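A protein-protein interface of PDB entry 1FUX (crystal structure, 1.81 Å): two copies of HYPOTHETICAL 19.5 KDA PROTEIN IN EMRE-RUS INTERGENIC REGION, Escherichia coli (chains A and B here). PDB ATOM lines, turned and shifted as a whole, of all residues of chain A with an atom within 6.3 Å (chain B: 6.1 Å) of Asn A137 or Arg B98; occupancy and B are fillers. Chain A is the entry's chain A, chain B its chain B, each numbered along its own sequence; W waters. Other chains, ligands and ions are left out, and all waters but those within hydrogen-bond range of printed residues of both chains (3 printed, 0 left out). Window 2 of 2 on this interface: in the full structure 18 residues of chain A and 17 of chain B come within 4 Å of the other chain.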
ATOM      1  N   GLN A  96      24.346 -28.434 -14.609  1.00  0.00           N
ATOM      2  CA  GLN A  96      24.283 -26.976 -14.447  1.00  0.00           C
ATOM      3  C   GLN A  96      23.248 -26.651 -13.362  1.00  0.00           C
ATOM      4  O   GLN A  96      22.190 -27.301 -13.313  1.00  0.00           O
ATOM      5  CB  GLN A  96      23.833 -26.301 -15.771  1.00  0.00           C
ATOM      6  CG  GLN A  96      24.732 -26.746 -16.957  1.00  0.00           C
ATOM      7  CD  GLN A  96      24.413 -25.944 -18.232  1.00  0.00           C
ATOM      8  OE1 GLN A  96      24.976 -24.877 -18.427  1.00  0.00           O
ATOM      9  NE2 GLN A  96      23.569 -26.443 -19.132  1.00  0.00           N
ATOM     10  N   GLY A  97      23.592 -25.708 -12.484  1.00  0.00           N
ATOM     11  CA  GLY A  97      22.723 -25.293 -11.404  1.00  0.00           C
ATOM     12  C   GLY A  97      21.843 -24.139 -11.948  1.00  0.00           C
ATOM     13  O   GLY A  97      22.033 -23.708 -13.081  1.00  0.00           O
ATOM     14  N   ARG A  98      20.920 -23.656 -11.125  1.00  0.00           N
ATOM     15  CA  ARG A  98      20.056 -22.574 -11.612  1.00  0.00           C
ATOM     16  C   ARG A  98      20.698 -21.202 -11.522  1.00  0.00           C
ATOM     17  O   ARG A  98      21.294 -20.891 -10.488  1.00  0.00           O
ATOM     18  CB  ARG A  98      18.845 -22.656 -10.648  1.00  0.00           C
ATOM     19  CG  ARG A  98      17.647 -21.873 -11.198  1.00  0.00           C
ATOM     20  CD  ARG A  98      16.612 -21.923 -10.084  1.00  0.00           C
ATOM     21  NE  ARG A  98      15.324 -21.470 -10.532  1.00  0.00           N
ATOM     22  CZ  ARG A  98      14.697 -20.337 -10.343  1.00  0.00           C
ATOM     23  NH1 ARG A  98      13.504 -20.404 -10.951  1.00  0.00           N
ATOM     24  NH2 ARG A  98      15.088 -19.274  -9.657  1.00  0.00           N
ATOM     25  N   ALA A 104      18.679 -23.275 -15.703  1.00  0.00           N
ATOM     26  CA  ALA A 104      19.930 -24.010 -15.564  1.00  0.00           C
ATOM     27  C   ALA A 104      20.749 -23.931 -16.868  1.00  0.00           C
ATOM     28  O   ALA A 104      20.607 -24.767 -17.743  1.00  0.00           O
ATOM     29  CB  ALA A 104      19.562 -25.462 -15.249  1.00  0.00           C
ATOM     30  N   VAL A 134      24.278 -31.450  -6.995  1.00  0.00           N
ATOM     31  CA  VAL A 134      23.618 -30.276  -7.551  1.00  0.00           C
ATOM     32  C   VAL A 134      22.692 -30.750  -8.670  1.00  0.00           C
ATOM     33  O   VAL A 134      22.899 -31.797  -9.298  1.00  0.00           O
ATOM     34  CB  VAL A 134      24.448 -29.064  -7.916  1.00  0.00           C
ATOM     35  CG1 VAL A 134      25.890 -29.117  -7.468  1.00  0.00           C
ATOM     36  CG2 VAL A 134      24.285 -28.485  -9.306  1.00  0.00           C
ATOM     37  N   ASP A 135      21.604 -29.996  -8.799  1.00  0.00           N
ATOM     38  CA  ASP A 135      20.666 -30.307  -9.871  1.00  0.00           C
ATOM     39  C   ASP A 135      20.205 -29.002 -10.487  1.00  0.00           C
ATOM     40  O   ASP A 135      20.674 -27.908 -10.107  1.00  0.00           O
ATOM     41  CB  ASP A 135      19.580 -31.246  -9.405  1.00  0.00           C
ATOM     42  CG  ASP A 135      18.709 -30.723  -8.286  1.00  0.00           C
ATOM     43  OD1 ASP A 135      18.513 -29.497  -8.130  1.00  0.00           O
ATOM     44  OD2 ASP A 135      18.185 -31.620  -7.562  1.00  0.00           O
ATOM     45  N   SER A 136      19.216 -29.077 -11.375  1.00  0.00           N
ATOM     46  CA  SER A 136      18.771 -27.860 -12.037  1.00  0.00           C
ATOM     47  C   SER A 136      18.090 -26.903 -11.087  1.00  0.00           C
ATOM     48  O   SER A 136      17.945 -25.747 -11.499  1.00  0.00           O
ATOM     49  CB  SER A 136      17.873 -28.181 -13.243  1.00  0.00           C
ATOM     50  OG  SER A 136      16.757 -28.867 -12.713  1.00  0.00           O
ATOM     51  N   ASN A 137      17.662 -27.357  -9.918  1.00  0.00           N
ATOM     52  CA  ASN A 137      17.016 -26.462  -8.973  1.00  0.00           C
ATOM     53  C   ASN A 137      18.027 -25.881  -7.979  1.00  0.00           C
ATOM     54  O   ASN A 137      17.594 -25.088  -7.133  1.00  0.00           O
ATOM     55  CB  ASN A 137      16.017 -27.294  -8.179  1.00  0.00           C
ATOM     56  CG  ASN A 137      14.761 -27.600  -8.971  1.00  0.00           C
ATOM     57  OD1 ASN A 137      14.193 -26.763  -9.696  1.00  0.00           O
ATOM     58  ND2 ASN A 137      14.335 -28.854  -8.767  1.00  0.00           N
ATOM     59  N   SER A 138      19.285 -26.264  -7.982  1.00  0.00           N
ATOM     60  CA  SER A 138      20.232 -25.731  -7.010  1.00  0.00           C
ATOM     61  C   SER A 138      20.510 -24.250  -7.216  1.00  0.00           C
ATOM     62  O   SER A 138      21.071 -23.885  -8.238  1.00  0.00           O
ATOM     63  CB  SER A 138      21.586 -26.490  -7.104  1.00  0.00           C
ATOM     64  OG  SER A 138      21.292 -27.863  -6.814  1.00  0.00           O
ATOM     65  N   SER A 139      20.171 -23.373  -6.245  1.00  0.00           N
ATOM     66  CA  SER A 139      20.475 -21.957  -6.443  1.00  0.00           C
ATOM     67  C   SER A 139      21.976 -21.687  -6.507  1.00  0.00           C
ATOM     68  O   SER A 139      22.795 -22.471  -6.005  1.00  0.00           O
ATOM     69  CB  SER A 139      19.930 -21.133  -5.244  1.00  0.00           C
ATOM     70  OG  SER A 139      20.702 -21.453  -4.098  1.00  0.00           O
ATOM     71  N   LEU A 142      23.599 -22.069  -3.089  1.00  0.00           N
ATOM     72  CA  LEU A 142      23.735 -23.451  -2.673  1.00  0.00           C
ATOM     73  C   LEU A 142      24.939 -24.076  -3.351  1.00  0.00           C
ATOM     74  O   LEU A 142      25.765 -24.745  -2.716  1.00  0.00           O
ATOM     75  CB  LEU A 142      22.481 -24.288  -2.941  1.00  0.00           C
ATOM     76  CG  LEU A 142      22.585 -25.789  -2.594  1.00  0.00           C
ATOM     77  CD1 LEU A 142      23.074 -25.965  -1.156  1.00  0.00           C
ATOM     78  CD2 LEU A 142      21.261 -26.522  -2.825  1.00  0.00           C
ATOM     79  N   TRP B  64      19.484 -15.997   0.641  1.00  0.00           N
ATOM     80  CA  TRP B  64      18.134 -15.412   0.705  1.00  0.00           C
ATOM     81  C   TRP B  64      17.178 -16.410   1.389  1.00  0.00           C
ATOM     82  O   TRP B  64      16.942 -17.532   0.928  1.00  0.00           O
ATOM     83  CB  TRP B  64      17.570 -15.285  -0.729  1.00  0.00           C
ATOM     84  CG  TRP B  64      18.224 -14.176  -1.499  1.00  0.00           C
ATOM     85  CD1 TRP B  64      19.128 -14.285  -2.515  1.00  0.00           C
ATOM     86  CD2 TRP B  64      18.016 -12.775  -1.280  1.00  0.00           C
ATOM     87  NE1 TRP B  64      19.521 -13.027  -2.931  1.00  0.00           N
ATOM     88  CE2 TRP B  64      18.821 -12.086  -2.203  1.00  0.00           C
ATOM     89  CE3 TRP B  64      17.200 -12.040  -0.407  1.00  0.00           C
ATOM     90  CZ2 TRP B  64      18.811 -10.708  -2.319  1.00  0.00           C
ATOM     91  CZ3 TRP B  64      17.206 -10.667  -0.491  1.00  0.00           C
ATOM     92  CH2 TRP B  64      18.032  -9.988  -1.430  1.00  0.00           C
ATOM     93  N   THR B  67      11.372 -14.115   0.517  1.00  0.00           N
ATOM     94  CA  THR B  67      11.008 -12.917  -0.201  1.00  0.00           C
ATOM     95  C   THR B  67       9.463 -12.956  -0.370  1.00  0.00           C
ATOM     96  O   THR B  67       8.858 -13.972  -0.674  1.00  0.00           O
ATOM     97  CB  THR B  67      11.606 -12.679  -1.578  1.00  0.00           C
ATOM     98  OG1 THR B  67      11.168 -13.711  -2.495  1.00  0.00           O
ATOM     99  CG2 THR B  67      13.125 -12.630  -1.529  1.00  0.00           C
ATOM    100  N   GLN B  96       5.163 -14.894  -2.997  1.00  0.00           N
ATOM    101  CA  GLN B  96       6.481 -15.271  -2.489  1.00  0.00           C
ATOM    102  C   GLN B  96       7.409 -15.655  -3.650  1.00  0.00           C
ATOM    103  O   GLN B  96       7.009 -16.410  -4.537  1.00  0.00           O
ATOM    104  CB  GLN B  96       6.365 -16.410  -1.491  1.00  0.00           C
ATOM    105  CG  GLN B  96       5.317 -16.028  -0.391  1.00  0.00           C
ATOM    106  CD  GLN B  96       5.383 -16.936   0.809  1.00  0.00           C
ATOM    107  OE1 GLN B  96       6.160 -16.828   1.757  1.00  0.00           O
ATOM    108  NE2 GLN B  96       4.596 -17.993   0.739  1.00  0.00           N
ATOM    109  N   GLY B  97       8.657 -15.201  -3.567  1.00  0.00           N
ATOM    110  CA  GLY B  97       9.698 -15.589  -4.524  1.00  0.00           C
ATOM    111  C   GLY B  97      10.412 -16.822  -3.962  1.00  0.00           C
ATOM    112  O   GLY B  97      10.201 -17.407  -2.864  1.00  0.00           O
ATOM    113  N   ARG B  98      11.365 -17.278  -4.788  1.00  0.00           N
ATOM    114  CA  ARG B  98      12.121 -18.481  -4.468  1.00  0.00           C
ATOM    115  C   ARG B  98      13.280 -18.156  -3.513  1.00  0.00           C
ATOM    116  O   ARG B  98      14.026 -17.191  -3.719  1.00  0.00           O
ATOM    117  CB  ARG B  98      12.624 -19.079  -5.806  1.00  0.00           C
ATOM    118  CG  ARG B  98      13.047 -20.532  -5.663  1.00  0.00           C
ATOM    119  CD  ARG B  98      13.258 -21.136  -7.081  1.00  0.00           C
ATOM    120  NE  ARG B  98      14.565 -21.724  -6.947  1.00  0.00           N
ATOM    121  CZ  ARG B  98      15.140 -22.870  -6.828  1.00  0.00           C
ATOM    122  NH1 ARG B  98      14.425 -23.977  -6.886  1.00  0.00           N
ATOM    123  NH2 ARG B  98      16.440 -22.934  -6.669  1.00  0.00           N
ATOM    124  N   ASN B  99      13.390 -18.860  -2.410  1.00  0.00           N
ATOM    125  CA  ASN B  99      14.520 -18.662  -1.495  1.00  0.00           C
ATOM    126  C   ASN B  99      15.697 -19.501  -1.948  1.00  0.00           C
ATOM    127  O   ASN B  99      15.620 -20.317  -2.913  1.00  0.00           O
ATOM    128  CB  ASN B  99      14.118 -18.926  -0.031  1.00  0.00           C
ATOM    129  CG  ASN B  99      13.731 -20.364   0.252  1.00  0.00           C
ATOM    130  OD1 ASN B  99      14.376 -21.252  -0.273  1.00  0.00           O
ATOM    131  ND2 ASN B  99      12.742 -20.623   1.124  1.00  0.00           N
ATOM    132  N   ASP B 100      16.849 -19.346  -1.283  1.00  0.00           N
ATOM    133  CA  ASP B 100      18.023 -20.123  -1.655  1.00  0.00           C
ATOM    134  C   ASP B 100      17.961 -21.592  -1.295  1.00  0.00           C
ATOM    135  O   ASP B 100      18.749 -22.411  -1.792  1.00  0.00           O
ATOM    136  CB  ASP B 100      19.336 -19.513  -1.198  1.00  0.00           C
ATOM    137  CG  ASP B 100      19.734 -18.371  -2.095  1.00  0.00           C
ATOM    138  OD1 ASP B 100      19.375 -18.256  -3.307  1.00  0.00           O
ATOM    139  OD2 ASP B 100      20.400 -17.444  -1.579  1.00  0.00           O
ATOM    140  N   PHE B 101      17.013 -21.973  -0.436  1.00  0.00           N
ATOM    141  CA  PHE B 101      16.782 -23.368  -0.154  1.00  0.00           C
ATOM    142  C   PHE B 101      16.051 -23.978  -1.361  1.00  0.00           C
ATOM    143  O   PHE B 101      16.020 -25.211  -1.381  1.00  0.00           O
ATOM    144  CB  PHE B 101      15.967 -23.644   1.098  1.00  0.00           C
ATOM    145  CG  PHE B 101      16.582 -23.035   2.342  1.00  0.00           C
ATOM    146  CD1 PHE B 101      16.069 -21.852   2.847  1.00  0.00           C
ATOM    147  CD2 PHE B 101      17.619 -23.679   3.003  1.00  0.00           C
ATOM    148  CE1 PHE B 101      16.621 -21.304   4.011  1.00  0.00           C
ATOM    149  CE2 PHE B 101      18.156 -23.160   4.175  1.00  0.00           C
ATOM    150  CZ  PHE B 101      17.662 -21.967   4.671  1.00  0.00           C
ATOM    151  N   GLY B 102      15.517 -23.202  -2.303  1.00  0.00           N
ATOM    152  CA  GLY B 102      14.917 -23.901  -3.439  1.00  0.00           C
ATOM    153  C   GLY B 102      13.412 -23.913  -3.380  1.00  0.00           C
ATOM    154  O   GLY B 102      12.807 -24.521  -4.294  1.00  0.00           O
ATOM    155  N   TYR B 103      12.786 -23.196  -2.464  1.00  0.00           N
ATOM    156  CA  TYR B 103      11.336 -23.113  -2.415  1.00  0.00           C
ATOM    157  C   TYR B 103      10.806 -21.703  -2.130  1.00  0.00           C
ATOM    158  O   TYR B 103      11.523 -20.807  -1.735  1.00  0.00           O
ATOM    159  CB  TYR B 103      10.676 -24.073  -1.442  1.00  0.00           C
ATOM    160  CG  TYR B 103      10.909 -23.781   0.043  1.00  0.00           C
ATOM    161  CD1 TYR B 103      10.024 -22.977   0.748  1.00  0.00           C
ATOM    162  CD2 TYR B 103      11.986 -24.329   0.687  1.00  0.00           C
ATOM    163  CE1 TYR B 103      10.208 -22.741   2.112  1.00  0.00           C
ATOM    164  CE2 TYR B 103      12.209 -24.094   2.039  1.00  0.00           C
ATOM    165  CZ  TYR B 103      11.302 -23.291   2.727  1.00  0.00           C
ATOM    166  OH  TYR B 103      11.553 -23.088   4.062  1.00  0.00           O
ATOM    167  N   ALA B 104       9.539 -21.479  -2.488  1.00  0.00           N
ATOM    168  CA  ALA B 104       8.885 -20.210  -2.353  1.00  0.00           C
ATOM    169  C   ALA B 104       8.215 -20.032  -0.986  1.00  0.00           C
ATOM    170  O   ALA B 104       7.064 -20.457  -0.824  1.00  0.00           O
ATOM    171  CB  ALA B 104       7.818 -20.037  -3.428  1.00  0.00           C
ATOM    172  N   GLY B 105       8.905 -19.390  -0.078  1.00  0.00           N
ATOM    173  CA  GLY B 105       8.343 -19.205   1.279  1.00  0.00           C
ATOM    174  C   GLY B 105       9.503 -18.943   2.220  1.00  0.00           C
ATOM    175  O   GLY B 105      10.674 -18.856   1.825  1.00  0.00           O
ATOM    176  N   ASP B 135       7.097 -14.371  -9.302  1.00  0.00           N
ATOM    177  CA  ASP B 135       6.364 -15.613  -9.015  1.00  0.00           C
ATOM    178  C   ASP B 135       7.268 -16.555  -8.235  1.00  0.00           C
ATOM    179  O   ASP B 135       8.382 -16.196  -7.799  1.00  0.00           O
ATOM    180  CB  ASP B 135       5.726 -16.242 -10.260  1.00  0.00           C
ATOM    181  CG  ASP B 135       6.710 -16.597 -11.346  1.00  0.00           C
ATOM    182  OD1 ASP B 135       7.904 -16.669 -11.018  1.00  0.00           O
ATOM    183  OD2 ASP B 135       6.353 -16.833 -12.529  1.00  0.00           O
ATOM    184  N   SER B 136       6.858 -17.829  -8.078  1.00  0.00           N
ATOM    185  CA  SER B 136       7.600 -18.839  -7.373  1.00  0.00           C
ATOM    186  C   SER B 136       8.907 -19.215  -8.073  1.00  0.00           C
ATOM    187  O   SER B 136       9.777 -19.739  -7.397  1.00  0.00           O
ATOM    188  CB  SER B 136       6.753 -20.118  -7.122  1.00  0.00           C
ATOM    189  OG  SER B 136       6.468 -20.694  -8.355  1.00  0.00           O
ATOM    190  N   ASN B 137       9.156 -18.750  -9.279  1.00  0.00           N
ATOM    191  CA  ASN B 137      10.438 -18.940  -9.941  1.00  0.00           C
ATOM    192  C   ASN B 137      11.413 -17.781  -9.761  1.00  0.00           C
ATOM    193  O   ASN B 137      12.565 -17.949 -10.165  1.00  0.00           O
ATOM    194  CB  ASN B 137      10.168 -19.068 -11.476  1.00  0.00           C
ATOM    195  CG  ASN B 137       9.757 -20.502 -11.827  1.00  0.00           C
ATOM    196  OD1 ASN B 137      10.089 -21.438 -11.117  1.00  0.00           O
ATOM    197  ND2 ASN B 137       9.040 -20.644 -12.928  1.00  0.00           N
ATOM    198  N   SER B 138      11.026 -16.658  -9.180  1.00  0.00           N
ATOM    199  CA  SER B 138      11.909 -15.515  -9.102  1.00  0.00           C
ATOM    200  C   SER B 138      12.990 -15.711  -8.064  1.00  0.00           C
ATOM    201  O   SER B 138      12.658 -15.840  -6.892  1.00  0.00           O
ATOM    202  CB  SER B 138      11.126 -14.216  -8.806  1.00  0.00           C
ATOM    203  OG  SER B 138      10.021 -14.126  -9.685  1.00  0.00           O
ATOM    204  N   SER B 139      14.244 -15.705  -8.527  1.00  0.00           N
ATOM    205  CA  SER B 139      15.339 -15.801  -7.571  1.00  0.00           C
ATOM    206  C   SER B 139      15.356 -14.623  -6.592  1.00  0.00           C
ATOM    207  O   SER B 139      14.758 -13.575  -6.883  1.00  0.00           O
ATOM    208  CB  SER B 139      16.683 -15.837  -8.300  1.00  0.00           C
ATOM    209  OG  SER B 139      16.966 -14.593  -8.916  1.00  0.00           O
ATOM    210  N   GLY B 140      16.108 -14.810  -5.506  1.00  0.00           N
ATOM    211  CA  GLY B 140      16.275 -13.680  -4.533  1.00  0.00           C
ATOM    212  C   GLY B 140      16.882 -12.470  -5.215  1.00  0.00           C
ATOM    213  O   GLY B 140      16.516 -11.326  -4.958  1.00  0.00           O
ATOM    214  N   VAL B 143      14.308 -10.594  -7.408  1.00  0.00           N
ATOM    215  CA  VAL B 143      13.447  -9.790  -6.535  1.00  0.00           C
ATOM    216  C   VAL B 143      14.183  -8.555  -6.026  1.00  0.00           C
ATOM    217  O   VAL B 143      13.644  -7.414  -5.997  1.00  0.00           O
ATOM    218  CB  VAL B 143      12.955 -10.643  -5.345  1.00  0.00           C
ATOM    219  CG1 VAL B 143      12.219  -9.777  -4.325  1.00  0.00           C
ATOM    220  CG2 VAL B 143      11.982 -11.739  -5.812  1.00  0.00           C
HETATM  221  O   HOH W   1      18.591 -24.123  -3.994  1.00  0.00           O
HETATM  222  O   HOH W   2      16.898 -19.266  -6.925  1.00  0.00           O
HETATM  223  O   HOH W   3      17.499 -26.648  -4.087  1.00  0.00           O
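Among the printed residues, pairs that only touch across the chains: Arg A98 with Arg B98 (3.6 Å), Arg A98 with Ser B139 (3.8 Å) and Ser A139 with Arg B98 (3.8 Å).
Water W1 lies within hydrogen-bond range of O of Asp B100, N of Ser A139 and O of Asn A137.
Water W2 bridges NH2 of Arg A98 (3.3 Å) and NE of Arg B98 (3.4 Å).
Water W3 bridges O of Phe B101 (3.4 Å) and O of Asn A137 (3.4 Å).
Printed residues of chain B within 4 Å of Arg A98: Arg B98 (3.6 Å), Asn B137 (2.7 Å) and Ser B139 (3.8 Å).
Gln B96 touches none of the printed residues of chain A.
Arg B98 touches three residues of chain A.
Of the printed residues of chain A, Asp B100 touches Ser A139.
Of the printed residues of chain A, Ser B139 touches Arg A98 (3.8 Å).
The nearest residue of chain A that does not touch Arg B98 is Ser A138 (4.3 Å).
The nearest printed residue of chain B that does not touch Arg A98 is Ser B138 (4.4 Å).
Of the 11 printed residues of chain A, 3 touch a printed residue of chain B.
Printed residues of chain B that touch a printed residue of chain A: Arg B98, Asp B100, Asn B137 and Ser B139.
Along chain B the printed residues that touch a printed residue of chain A span positions 98 to 139.
Arg B98 touches its own counterpart, Arg A98.
Arg A98 touches Asn B137, and with the chains exchanged Asn A137 touches Arg B98.
Arg A98 touches Ser B139, and with the chains exchanged Ser A139 touches Arg B98.
9 positions are printed for both chains.
Of the 6 pairs that touch across the chains among the printed residues, 5 have their exchanged pair printed and touching as well.
The guanidinium group of Arg A98 is in hydrogen-bond range of the backbone carbonyl oxygen of Asn B137 (2.7 Å).
The backbone carbonyl oxygen (O) of Asn A137 sits at hydrogen-bond distance from the guanidinium group (NH2) of Arg B98 (2.5 Å).
OG of Ser A139 is in hydrogen-bond range of O of Asp B100, 3.2 Å away.
The backbone NH (N) of Arg A98 sits at hydrogen-bond distance from the backbone carbonyl oxygen (O) of Ser A138 (2.9 Å).
The side-chain hydroxyl of Ser A139 lies within hydrogen-bond range of the backbone NH of Leu A142 (3.1 Å).
The backbone NH (N) of Trp B64 lies within hydrogen-bond range of the side-chain carboxylate (OD2) of Asp B100, 2.8 Å away.
The guanidinium group (NH1) of Arg B98 is in hydrogen-bond range of the backbone carbonyl oxygen (O) of Gly B102, 3.1 Å away.
N of Arg B98 sits at hydrogen-bond distance from O of Ser B138, at 2.9 Å.
The backbone NH (N) of Asn B137 lies within hydrogen-bond range of the side-chain carboxylate (OD1) of Asp B135.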
